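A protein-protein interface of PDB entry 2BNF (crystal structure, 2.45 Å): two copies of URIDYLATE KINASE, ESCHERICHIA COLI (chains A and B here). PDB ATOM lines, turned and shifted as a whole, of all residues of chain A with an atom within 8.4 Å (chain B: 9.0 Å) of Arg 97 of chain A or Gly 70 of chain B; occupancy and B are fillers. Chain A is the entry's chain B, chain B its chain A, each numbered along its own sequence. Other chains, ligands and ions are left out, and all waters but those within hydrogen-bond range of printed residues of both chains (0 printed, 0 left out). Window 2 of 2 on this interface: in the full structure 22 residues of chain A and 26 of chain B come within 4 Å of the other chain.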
ATOM      1  N   ALA A  31      21.566 -33.264   9.895  1.00  0.00           N
ATOM      2  CA  ALA A  31      22.989 -33.000   9.730  1.00  0.00           C
ATOM      3  C   ALA A  31      23.616 -33.504   8.438  1.00  0.00           C
ATOM      4  O   ALA A  31      24.461 -32.822   7.865  1.00  0.00           O
ATOM      5  CB  ALA A  31      23.758 -33.570  10.922  1.00  0.00           C
ATOM      6  N   SER A  32      23.222 -34.693   7.983  1.00  0.00           N
ATOM      7  CA  SER A  32      23.801 -35.258   6.764  1.00  0.00           C
ATOM      8  C   SER A  32      23.299 -34.588   5.491  1.00  0.00           C
ATOM      9  O   SER A  32      23.970 -34.608   4.466  1.00  0.00           O
ATOM     10  CB  SER A  32      23.547 -36.766   6.695  1.00  0.00           C
ATOM     11  OG  SER A  32      22.170 -37.050   6.567  1.00  0.00           O
ATOM     12  N   LEU A  34      22.547 -31.433   5.582  1.00  0.00           N
ATOM     13  CA  LEU A  34      23.204 -30.144   5.729  1.00  0.00           C
ATOM     14  C   LEU A  34      24.630 -30.209   5.178  1.00  0.00           C
ATOM     15  O   LEU A  34      25.095 -29.274   4.522  1.00  0.00           O
ATOM     16  CB  LEU A  34      23.239 -29.751   7.206  1.00  0.00           C
ATOM     17  CG  LEU A  34      23.251 -28.253   7.494  1.00  0.00           C
ATOM     18  CD1 LEU A  34      21.932 -27.652   7.061  1.00  0.00           C
ATOM     19  CD2 LEU A  34      23.469 -28.019   8.980  1.00  0.00           C
ATOM     20  N   ASP A  35      25.320 -31.313   5.447  1.00  0.00           N
ATOM     21  CA  ASP A  35      26.688 -31.489   4.967  1.00  0.00           C
ATOM     22  C   ASP A  35      26.741 -31.709   3.464  1.00  0.00           C
ATOM     23  O   ASP A  35      27.732 -31.379   2.823  1.00  0.00           O
ATOM     24  CB  ASP A  35      27.366 -32.661   5.680  1.00  0.00           C
ATOM     25  CG  ASP A  35      27.805 -32.316   7.093  1.00  0.00           C
ATOM     26  OD1 ASP A  35      28.125 -33.253   7.851  1.00  0.00           O
ATOM     27  OD2 ASP A  35      27.837 -31.114   7.450  1.00  0.00           O
ATOM     28  N   ALA A  38      26.328 -28.301   1.897  1.00  0.00           N
ATOM     29  CA  ALA A  38      27.584 -27.570   1.925  1.00  0.00           C
ATOM     30  C   ALA A  38      28.469 -27.978   0.759  1.00  0.00           C
ATOM     31  O   ALA A  38      28.944 -27.122   0.019  1.00  0.00           O
ATOM     32  CB  ALA A  38      28.302 -27.812   3.245  1.00  0.00           C
ATOM     33  N   GLN A  39      28.681 -29.281   0.589  1.00  0.00           N
ATOM     34  CA  GLN A  39      29.512 -29.787  -0.496  1.00  0.00           C
ATOM     35  C   GLN A  39      29.064 -29.292  -1.866  1.00  0.00           C
ATOM     36  O   GLN A  39      29.882 -28.910  -2.690  1.00  0.00           O
ATOM     37  CB  GLN A  39      29.515 -31.319  -0.492  1.00  0.00           C
ATOM     38  CG  GLN A  39      30.345 -31.954   0.619  1.00  0.00           C
ATOM     39  CD  GLN A  39      31.776 -31.443   0.646  1.00  0.00           C
ATOM     40  OE1 GLN A  39      32.431 -31.330  -0.387  1.00  0.00           O
ATOM     41  NE2 GLN A  39      32.269 -31.146   1.835  1.00  0.00           N
ATOM     42  N   LYS A  42      29.766 -25.757  -2.208  1.00  0.00           N
ATOM     43  CA  LYS A  42      31.208 -25.590  -2.309  1.00  0.00           C
ATOM     44  C   LYS A  42      31.601 -25.592  -3.774  1.00  0.00           C
ATOM     45  O   LYS A  42      32.379 -24.753  -4.233  1.00  0.00           O
ATOM     46  CB  LYS A  42      31.922 -26.728  -1.594  1.00  0.00           C
ATOM     47  CG  LYS A  42      33.441 -26.617  -1.619  1.00  0.00           C
ATOM     48  CD  LYS A  42      34.072 -27.673  -0.737  1.00  0.00           C
ATOM     49  CE  LYS A  42      35.548 -27.397  -0.505  1.00  0.00           C
ATOM     50  NZ  LYS A  42      36.119 -28.344   0.502  1.00  0.00           N
ATOM     51  N   LEU A  89      22.128 -20.419  10.751  1.00  0.00           N
ATOM     52  CA  LEU A  89      23.292 -20.636  11.616  1.00  0.00           C
ATOM     53  C   LEU A  89      23.846 -22.054  11.421  1.00  0.00           C
ATOM     54  O   LEU A  89      25.055 -22.250  11.361  1.00  0.00           O
ATOM     55  CB  LEU A  89      22.872 -20.419  13.067  1.00  0.00           C
ATOM     56  CG  LEU A  89      23.879 -20.233  14.193  1.00  0.00           C
ATOM     57  CD1 LEU A  89      24.901 -19.158  13.842  1.00  0.00           C
ATOM     58  CD2 LEU A  89      23.103 -19.833  15.446  1.00  0.00           C
ATOM     59  N   ALA A  90      22.959 -23.043  11.325  1.00  0.00           N
ATOM     60  CA  ALA A  90      23.391 -24.413  11.111  1.00  0.00           C
ATOM     61  C   ALA A  90      24.012 -24.514   9.715  1.00  0.00           C
ATOM     62  O   ALA A  90      25.053 -25.128   9.541  1.00  0.00           O
ATOM     63  CB  ALA A  90      22.212 -25.359  11.234  1.00  0.00           C
ATOM     64  N   MET A  91      23.374 -23.894   8.722  1.00  0.00           N
ATOM     65  CA  MET A  91      23.883 -23.929   7.357  1.00  0.00           C
ATOM     66  C   MET A  91      25.281 -23.313   7.297  1.00  0.00           C
ATOM     67  O   MET A  91      26.201 -23.914   6.762  1.00  0.00           O
ATOM     68  CB  MET A  91      22.923 -23.193   6.411  1.00  0.00           C
ATOM     69  CG  MET A  91      23.346 -23.174   4.930  1.00  0.00           C
ATOM     70  SD  MET A  91      23.583 -24.922   4.081  1.00  0.00           S
ATOM     71  CE  MET A  91      21.763 -25.531   4.176  1.00  0.00           C
ATOM     72  N   ARG A  92      25.437 -22.120   7.865  1.00  0.00           N
ATOM     73  CA  ARG A  92      26.725 -21.440   7.877  1.00  0.00           C
ATOM     74  C   ARG A  92      27.809 -22.342   8.455  1.00  0.00           C
ATOM     75  O   ARG A  92      28.879 -22.494   7.864  1.00  0.00           O
ATOM     76  CB  ARG A  92      26.670 -20.155   8.712  1.00  0.00           C
ATOM     77  CG  ARG A  92      27.978 -19.369   8.655  1.00  0.00           C
ATOM     78  CD  ARG A  92      28.099 -18.356   9.768  1.00  0.00           C
ATOM     79  NE  ARG A  92      28.295 -18.993  11.068  1.00  0.00           N
ATOM     80  CZ  ARG A  92      28.317 -18.337  12.224  1.00  0.00           C
ATOM     81  NH1 ARG A  92      28.151 -17.022  12.243  1.00  0.00           N
ATOM     82  NH2 ARG A  92      28.502 -18.993  13.359  1.00  0.00           N
ATOM     83  N   ASP A  93      27.533 -22.936   9.614  1.00  0.00           N
ATOM     84  CA  ASP A  93      28.510 -23.805  10.239  1.00  0.00           C
ATOM     85  C   ASP A  93      28.899 -24.995   9.352  1.00  0.00           C
ATOM     86  O   ASP A  93      30.076 -25.361   9.285  1.00  0.00           O
ATOM     87  CB  ASP A  93      28.004 -24.314  11.584  1.00  0.00           C
ATOM     88  CG  ASP A  93      29.086 -25.023  12.359  1.00  0.00           C
ATOM     89  OD1 ASP A  93      30.049 -24.345  12.791  1.00  0.00           O
ATOM     90  OD2 ASP A  93      28.987 -26.254  12.515  1.00  0.00           O
ATOM     91  N   ALA A  94      27.920 -25.599   8.683  1.00  0.00           N
ATOM     92  CA  ALA A  94      28.197 -26.725   7.794  1.00  0.00           C
ATOM     93  C   ALA A  94      29.121 -26.252   6.676  1.00  0.00           C
ATOM     94  O   ALA A  94      29.947 -27.009   6.169  1.00  0.00           O
ATOM     95  CB  ALA A  94      26.898 -27.255   7.190  1.00  0.00           C
ATOM     96  N   LEU A  95      28.953 -24.989   6.298  1.00  0.00           N
ATOM     97  CA  LEU A  95      29.739 -24.369   5.240  1.00  0.00           C
ATOM     98  C   LEU A  95      31.162 -24.136   5.728  1.00  0.00           C
ATOM     99  O   LEU A  95      32.134 -24.445   5.032  1.00  0.00           O
ATOM    100  CB  LEU A  95      29.092 -23.037   4.814  1.00  0.00           C
ATOM    101  CG  LEU A  95      28.424 -22.891   3.438  1.00  0.00           C
ATOM    102  CD1 LEU A  95      27.937 -24.222   2.907  1.00  0.00           C
ATOM    103  CD2 LEU A  95      27.275 -21.918   3.556  1.00  0.00           C
ATOM    104  N   HIS A  96      31.298 -23.591   6.926  1.00  0.00           N
ATOM    105  CA  HIS A  96      32.632 -23.355   7.458  1.00  0.00           C
ATOM    106  C   HIS A  96      33.388 -24.672   7.599  1.00  0.00           C
ATOM    107  O   HIS A  96      34.553 -24.759   7.234  1.00  0.00           O
ATOM    108  CB  HIS A  96      32.540 -22.643   8.798  1.00  0.00           C
ATOM    109  CG  HIS A  96      32.165 -21.201   8.685  1.00  0.00           C
ATOM    110  ND1 HIS A  96      31.853 -20.424   9.779  1.00  0.00           N
ATOM    111  CD2 HIS A  96      32.075 -20.386   7.607  1.00  0.00           C
ATOM    112  CE1 HIS A  96      31.588 -19.192   9.381  1.00  0.00           C
ATOM    113  NE2 HIS A  96      31.717 -19.143   8.066  1.00  0.00           N
ATOM    114  N   ARG A  97      32.720 -25.708   8.100  1.00  0.00           N
ATOM    115  CA  ARG A  97      33.373 -27.004   8.284  1.00  0.00           C
ATOM    116  C   ARG A  97      33.774 -27.695   6.988  1.00  0.00           C
ATOM    117  O   ARG A  97      34.565 -28.648   6.998  1.00  0.00           O
ATOM    118  CB  ARG A  97      32.504 -27.934   9.134  1.00  0.00           C
ATOM    119  CG  ARG A  97      32.598 -27.639  10.604  1.00  0.00           C
ATOM    120  CD  ARG A  97      31.733 -28.563  11.454  1.00  0.00           C
ATOM    121  NE  ARG A  97      30.310 -28.263  11.355  1.00  0.00           N
ATOM    122  CZ  ARG A  97      29.426 -28.987  10.676  1.00  0.00           C
ATOM    123  NH1 ARG A  97      29.803 -30.074  10.019  1.00  0.00           N
ATOM    124  NH2 ARG A  97      28.152 -28.616  10.661  1.00  0.00           N
ATOM    125  N   ALA A  98      33.231 -27.208   5.876  1.00  0.00           N
ATOM    126  CA  ALA A  98      33.540 -27.738   4.552  1.00  0.00           C
ATOM    127  C   ALA A  98      34.517 -26.753   3.907  1.00  0.00           C
ATOM    128  O   ALA A  98      34.720 -26.741   2.701  1.00  0.00           O
ATOM    129  CB  ALA A  98      32.261 -27.856   3.715  1.00  0.00           C
ATOM    130  N   TYR A  99      35.101 -25.904   4.743  1.00  0.00           N
ATOM    131  CA  TYR A  99      36.085 -24.922   4.310  1.00  0.00           C
ATOM    132  C   TYR A  99      35.578 -23.962   3.250  1.00  0.00           C
ATOM    133  O   TYR A  99      36.269 -23.667   2.273  1.00  0.00           O
ATOM    134  CB  TYR A  99      37.335 -25.663   3.838  1.00  0.00           C
ATOM    135  CG  TYR A  99      37.842 -26.607   4.907  1.00  0.00           C
ATOM    136  CD1 TYR A  99      38.462 -26.112   6.057  1.00  0.00           C
ATOM    137  CD2 TYR A  99      37.610 -27.989   4.822  1.00  0.00           C
ATOM    138  CE1 TYR A  99      38.829 -26.960   7.097  1.00  0.00           C
ATOM    139  CE2 TYR A  99      37.975 -28.847   5.863  1.00  0.00           C
ATOM    140  CZ  TYR A  99      38.582 -28.319   6.996  1.00  0.00           C
ATOM    141  OH  TYR A  99      38.935 -29.141   8.043  1.00  0.00           O
ATOM    142  N   VAL A 100      34.360 -23.475   3.448  1.00  0.00           N
ATOM    143  CA  VAL A 100      33.762 -22.515   2.531  1.00  0.00           C
ATOM    144  C   VAL A 100      33.524 -21.209   3.283  1.00  0.00           C
ATOM    145  O   VAL A 100      32.980 -21.203   4.386  1.00  0.00           O
ATOM    146  CB  VAL A 100      32.423 -23.031   1.973  1.00  0.00           C
ATOM    147  CG1 VAL A 100      31.852 -22.040   0.971  1.00  0.00           C
ATOM    148  CG2 VAL A 100      32.626 -24.348   1.316  1.00  0.00           C
ATOM    149  N   ASN A 101      33.963 -20.104   2.700  1.00  0.00           N
ATOM    150  CA  ASN A 101      33.777 -18.802   3.322  1.00  0.00           C
ATOM    151  C   ASN A 101      32.294 -18.466   3.265  1.00  0.00           C
ATOM    152  O   ASN A 101      31.693 -18.459   2.187  1.00  0.00           O
ATOM    153  CB  ASN A 101      34.557 -17.730   2.561  1.00  0.00           C
ATOM    154  CG  ASN A 101      36.071 -17.905   2.667  1.00  0.00           C
ATOM    155  OD1 ASN A 101      36.809 -17.554   1.736  1.00  0.00           O
ATOM    156  ND2 ASN A 101      36.541 -18.425   3.804  1.00  0.00           N
ATOM    157  N   ALA A 102      31.700 -18.202   4.423  1.00  0.00           N
ATOM    158  CA  ALA A 102      30.288 -17.842   4.480  1.00  0.00           C
ATOM    159  C   ALA A 102      30.003 -16.869   5.614  1.00  0.00           C
ATOM    160  O   ALA A 102      30.684 -16.878   6.652  1.00  0.00           O
ATOM    161  CB  ALA A 102      29.437 -19.079   4.641  1.00  0.00           C
ATOM    162  N   GLY B  63      23.186 -28.056  22.543  1.00  0.00           N
ATOM    163  CA  GLY B  63      24.501 -27.921  21.939  1.00  0.00           C
ATOM    164  C   GLY B  63      25.346 -29.178  21.900  1.00  0.00           C
ATOM    165  O   GLY B  63      25.940 -29.500  20.869  1.00  0.00           O
ATOM    166  N   ALA B  64      25.418 -29.883  23.024  1.00  0.00           N
ATOM    167  CA  ALA B  64      26.200 -31.112  23.106  1.00  0.00           C
ATOM    168  C   ALA B  64      25.659 -32.129  22.112  1.00  0.00           C
ATOM    169  O   ALA B  64      26.429 -32.796  21.415  1.00  0.00           O
ATOM    170  CB  ALA B  64      26.144 -31.679  24.517  1.00  0.00           C
ATOM    171  N   GLY B  65      24.330 -32.232  22.063  1.00  0.00           N
ATOM    172  CA  GLY B  65      23.661 -33.151  21.157  1.00  0.00           C
ATOM    173  C   GLY B  65      23.989 -32.834  19.716  1.00  0.00           C
ATOM    174  O   GLY B  65      24.242 -33.739  18.926  1.00  0.00           O
ATOM    175  N   LEU B  66      23.989 -31.551  19.370  1.00  0.00           N
ATOM    176  CA  LEU B  66      24.314 -31.121  18.013  1.00  0.00           C
ATOM    177  C   LEU B  66      25.801 -31.386  17.707  1.00  0.00           C
ATOM    178  O   LEU B  66      26.149 -31.839  16.612  1.00  0.00           O
ATOM    179  CB  LEU B  66      24.002 -29.628  17.842  1.00  0.00           C
ATOM    180  CG  LEU B  66      22.529 -29.197  17.862  1.00  0.00           C
ATOM    181  CD1 LEU B  66      22.428 -27.699  18.077  1.00  0.00           C
ATOM    182  CD2 LEU B  66      21.849 -29.607  16.563  1.00  0.00           C
ATOM    183  N   ALA B  67      26.669 -31.104  18.678  1.00  0.00           N
ATOM    184  CA  ALA B  67      28.104 -31.313  18.507  1.00  0.00           C
ATOM    185  C   ALA B  67      28.424 -32.777  18.189  1.00  0.00           C
ATOM    186  O   ALA B  67      29.356 -33.067  17.439  1.00  0.00           O
ATOM    187  CB  ALA B  67      28.856 -30.862  19.756  1.00  0.00           C
ATOM    188  N   LYS B  68      27.658 -33.701  18.754  1.00  0.00           N
ATOM    189  CA  LYS B  68      27.888 -35.113  18.472  1.00  0.00           C
ATOM    190  C   LYS B  68      27.630 -35.364  16.996  1.00  0.00           C
ATOM    191  O   LYS B  68      28.294 -36.191  16.373  1.00  0.00           O
ATOM    192  CB  LYS B  68      26.951 -36.013  19.288  1.00  0.00           C
ATOM    193  CG  LYS B  68      27.345 -36.220  20.741  1.00  0.00           C
ATOM    194  CD  LYS B  68      26.501 -37.330  21.365  1.00  0.00           C
ATOM    195  CE  LYS B  68      26.818 -37.530  22.841  1.00  0.00           C
ATOM    196  NZ  LYS B  68      26.473 -36.331  23.657  1.00  0.00           N
ATOM    197  N   ALA B  69      26.660 -34.642  16.441  1.00  0.00           N
ATOM    198  CA  ALA B  69      26.301 -34.799  15.039  1.00  0.00           C
ATOM    199  C   ALA B  69      27.327 -34.201  14.078  1.00  0.00           C
ATOM    200  O   ALA B  69      27.142 -34.270  12.868  1.00  0.00           O
ATOM    201  CB  ALA B  69      24.920 -34.199  14.786  1.00  0.00           C
ATOM    202  N   GLY B  70      28.403 -33.621  14.617  1.00  0.00           N
ATOM    203  CA  GLY B  70      29.454 -33.044  13.786  1.00  0.00           C
ATOM    204  C   GLY B  70      29.636 -31.533  13.877  1.00  0.00           C
ATOM    205  O   GLY B  70      30.709 -31.006  13.580  1.00  0.00           O
ATOM    206  N   MET B  71      28.588 -30.839  14.304  1.00  0.00           N
ATOM    207  CA  MET B  71      28.584 -29.382  14.420  1.00  0.00           C
ATOM    208  C   MET B  71      29.528 -28.776  15.460  1.00  0.00           C
ATOM    209  O   MET B  71      29.890 -29.425  16.439  1.00  0.00           O
ATOM    210  CB  MET B  71      27.157 -28.927  14.705  1.00  0.00           C
ATOM    211  CG  MET B  71      26.941 -27.439  14.676  1.00  0.00           C
ATOM    212  SD  MET B  71      25.054 -27.093  14.629  1.00  0.00           S
ATOM    213  CE  MET B  71      24.714 -27.685  12.823  1.00  0.00           C
ATOM    214  N   ASN B  72      29.928 -27.524  15.244  1.00  0.00           N
ATOM    215  CA  ASN B  72      30.808 -26.841  16.190  1.00  0.00           C
ATOM    216  C   ASN B  72      30.047 -26.583  17.496  1.00  0.00           C
ATOM    217  O   ASN B  72      29.047 -25.879  17.516  1.00  0.00           O
ATOM    218  CB  ASN B  72      31.307 -25.518  15.591  1.00  0.00           C
ATOM    219  CG  ASN B  72      32.418 -25.718  14.557  1.00  0.00           C
ATOM    220  OD1 ASN B  72      33.477 -26.269  14.864  1.00  0.00           O
ATOM    221  ND2 ASN B  72      32.183 -25.259  13.330  1.00  0.00           N
ATOM    222  N   ARG B  73      30.526 -27.158  18.587  1.00  0.00           N
ATOM    223  CA  ARG B  73      29.878 -27.015  19.883  1.00  0.00           C
ATOM    224  C   ARG B  73      29.372 -25.606  20.203  1.00  0.00           C
ATOM    225  O   ARG B  73      28.250 -25.439  20.661  1.00  0.00           O
ATOM    226  CB  ARG B  73      30.822 -27.491  20.996  1.00  0.00           C
ATOM    227  CG  ARG B  73      30.221 -27.395  22.393  1.00  0.00           C
ATOM    228  CD  ARG B  73      28.823 -28.005  22.414  1.00  0.00           C
ATOM    229  NE  ARG B  73      28.158 -27.837  23.698  1.00  0.00           N
ATOM    230  CZ  ARG B  73      28.618 -28.335  24.840  1.00  0.00           C
ATOM    231  NH1 ARG B  73      29.744 -29.035  24.849  1.00  0.00           N
ATOM    232  NH2 ARG B  73      27.956 -28.128  25.968  1.00  0.00           N
ATOM    233  N   VAL B  75      28.551 -23.196  18.159  1.00  0.00           N
ATOM    234  CA  VAL B  75      27.424 -22.858  17.306  1.00  0.00           C
ATOM    235  C   VAL B  75      26.184 -23.624  17.771  1.00  0.00           C
ATOM    236  O   VAL B  75      25.064 -23.124  17.677  1.00  0.00           O
ATOM    237  CB  VAL B  75      27.721 -23.194  15.836  1.00  0.00           C
ATOM    238  CG1 VAL B  75      26.468 -23.013  14.998  1.00  0.00           C
ATOM    239  CG2 VAL B  75      28.827 -22.291  15.323  1.00  0.00           C
ATOM    240  N   GLY B  76      26.403 -24.839  18.272  1.00  0.00           N
ATOM    241  CA  GLY B  76      25.314 -25.657  18.767  1.00  0.00           C
ATOM    242  C   GLY B  76      24.701 -25.016  19.999  1.00  0.00           C
ATOM    243  O   GLY B  76      23.479 -25.040  20.197  1.00  0.00           O
ATOM    244  N   MET B  79      22.506 -22.018  18.989  1.00  0.00           N
ATOM    245  CA  MET B  79      21.208 -22.437  18.505  1.00  0.00           C
ATOM    246  C   MET B  79      20.352 -22.836  19.699  1.00  0.00           C
ATOM    247  O   MET B  79      19.159 -22.559  19.734  1.00  0.00           O
ATOM    248  CB  MET B  79      21.368 -23.601  17.525  1.00  0.00           C
ATOM    249  CG  MET B  79      21.831 -23.155  16.137  1.00  0.00           C
ATOM    250  SD  MET B  79      22.331 -24.614  14.973  1.00  0.00           S
ATOM    251  CE  MET B  79      20.552 -25.178  14.462  1.00  0.00           C
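The backbone NH of Asn 72 of chain B sits at hydrogen-bond distance from the side-chain carboxylate of Asp 93 of chain A (3.2 Å).
OD2 of Asp 35 of chain A is in salt-bridge range of NH1 of Arg 97 of chain A (3.4 Å).
OD2 of Asp 93 of chain A is in salt-bridge range of NE of Arg 97 of chain A, 2.7 Å away.
Among the printed residues, merely in contact across the chains: Asp 93 of chain A with Met 71 of chain B (3.2 Å), Arg 97 of chain A with Gly 70 of chain B (3.4 Å), Asp 93 of chain A with Val 75 of chain B (3.5 Å), Leu 89 of chain A with Met 79 of chain B (3.6 Å), Ala 90 of chain A with Met 79 of chain B (3.6 Å), Arg 97 of chain A with Asn 72 of chain B (3.6 Å), Arg 97 of chain A with Met 71 of chain B (3.7 Å), Ala 90 of chain A with Met 71 of chain B (3.8 Å), Arg 92 of chain A with Val 75 of chain B (3.9 Å), Leu 89 of chain A with Val 75 of chain B (3.9 Å) and Ala 31 of chain A with Ala 69 of chain B (3.97 Å).
Of chain A, only Arg 97 (3.4 Å) comes within 4 Å of Gly 70 of chain B.
No residue of chain B comes within 4 Å of Ala 94 of chain A.
No residue of chain B comes within 4 Å of Ala 98 of chain A.
Ala 69 of chain B touches just one residue of chain A: Ala 31.
Of the printed residues of chain B, Ala 90 of chain A touches Met 71 and Met 79.
Of the printed residues of chain A, Met 71 of chain B touches Ala 90, Asp 93 and Arg 97.
Of the printed residues of chain A, Met 79 of chain B touches Leu 89 and Ala 90.
Printed residues of chain B within 4 Å of Arg 92 of chain A: Val 75 (3.9 Å).
Arg 73 of chain B touches none of the printed residues of chain A.
Leu 66 of chain B touches none of the printed residues of chain A.
The nearest residue of chain B that does not touch Arg 97 of chain A is Ala 69 of chain B (5.7 Å).
The nearest printed residue of chain B that does not touch Ala 90 of chain A is Val 75 of chain B (5.1 Å).
Of the 21 printed residues of chain A, 6 touch a printed residue of chain B.
Hydrophobic or aromatic side chains of chain A within 4 Å of the printed part of chain B: Ala 31, Leu 89 and Ala 90.
Along chain A the printed residues that touch a printed residue of chain B span positions 31 to 97.
Printed residues of chain B that touch a printed residue of chain A: Ala 69, Gly 70, Met 71, Asn 72, Val 75 and Met 79.
Among the printed residues, 12 pairs touch across the chains.
No position is printed for both chains.
Of the 12 pairs that touch across the chains among the printed residues, none has its exchanged pair printed and touching as well.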
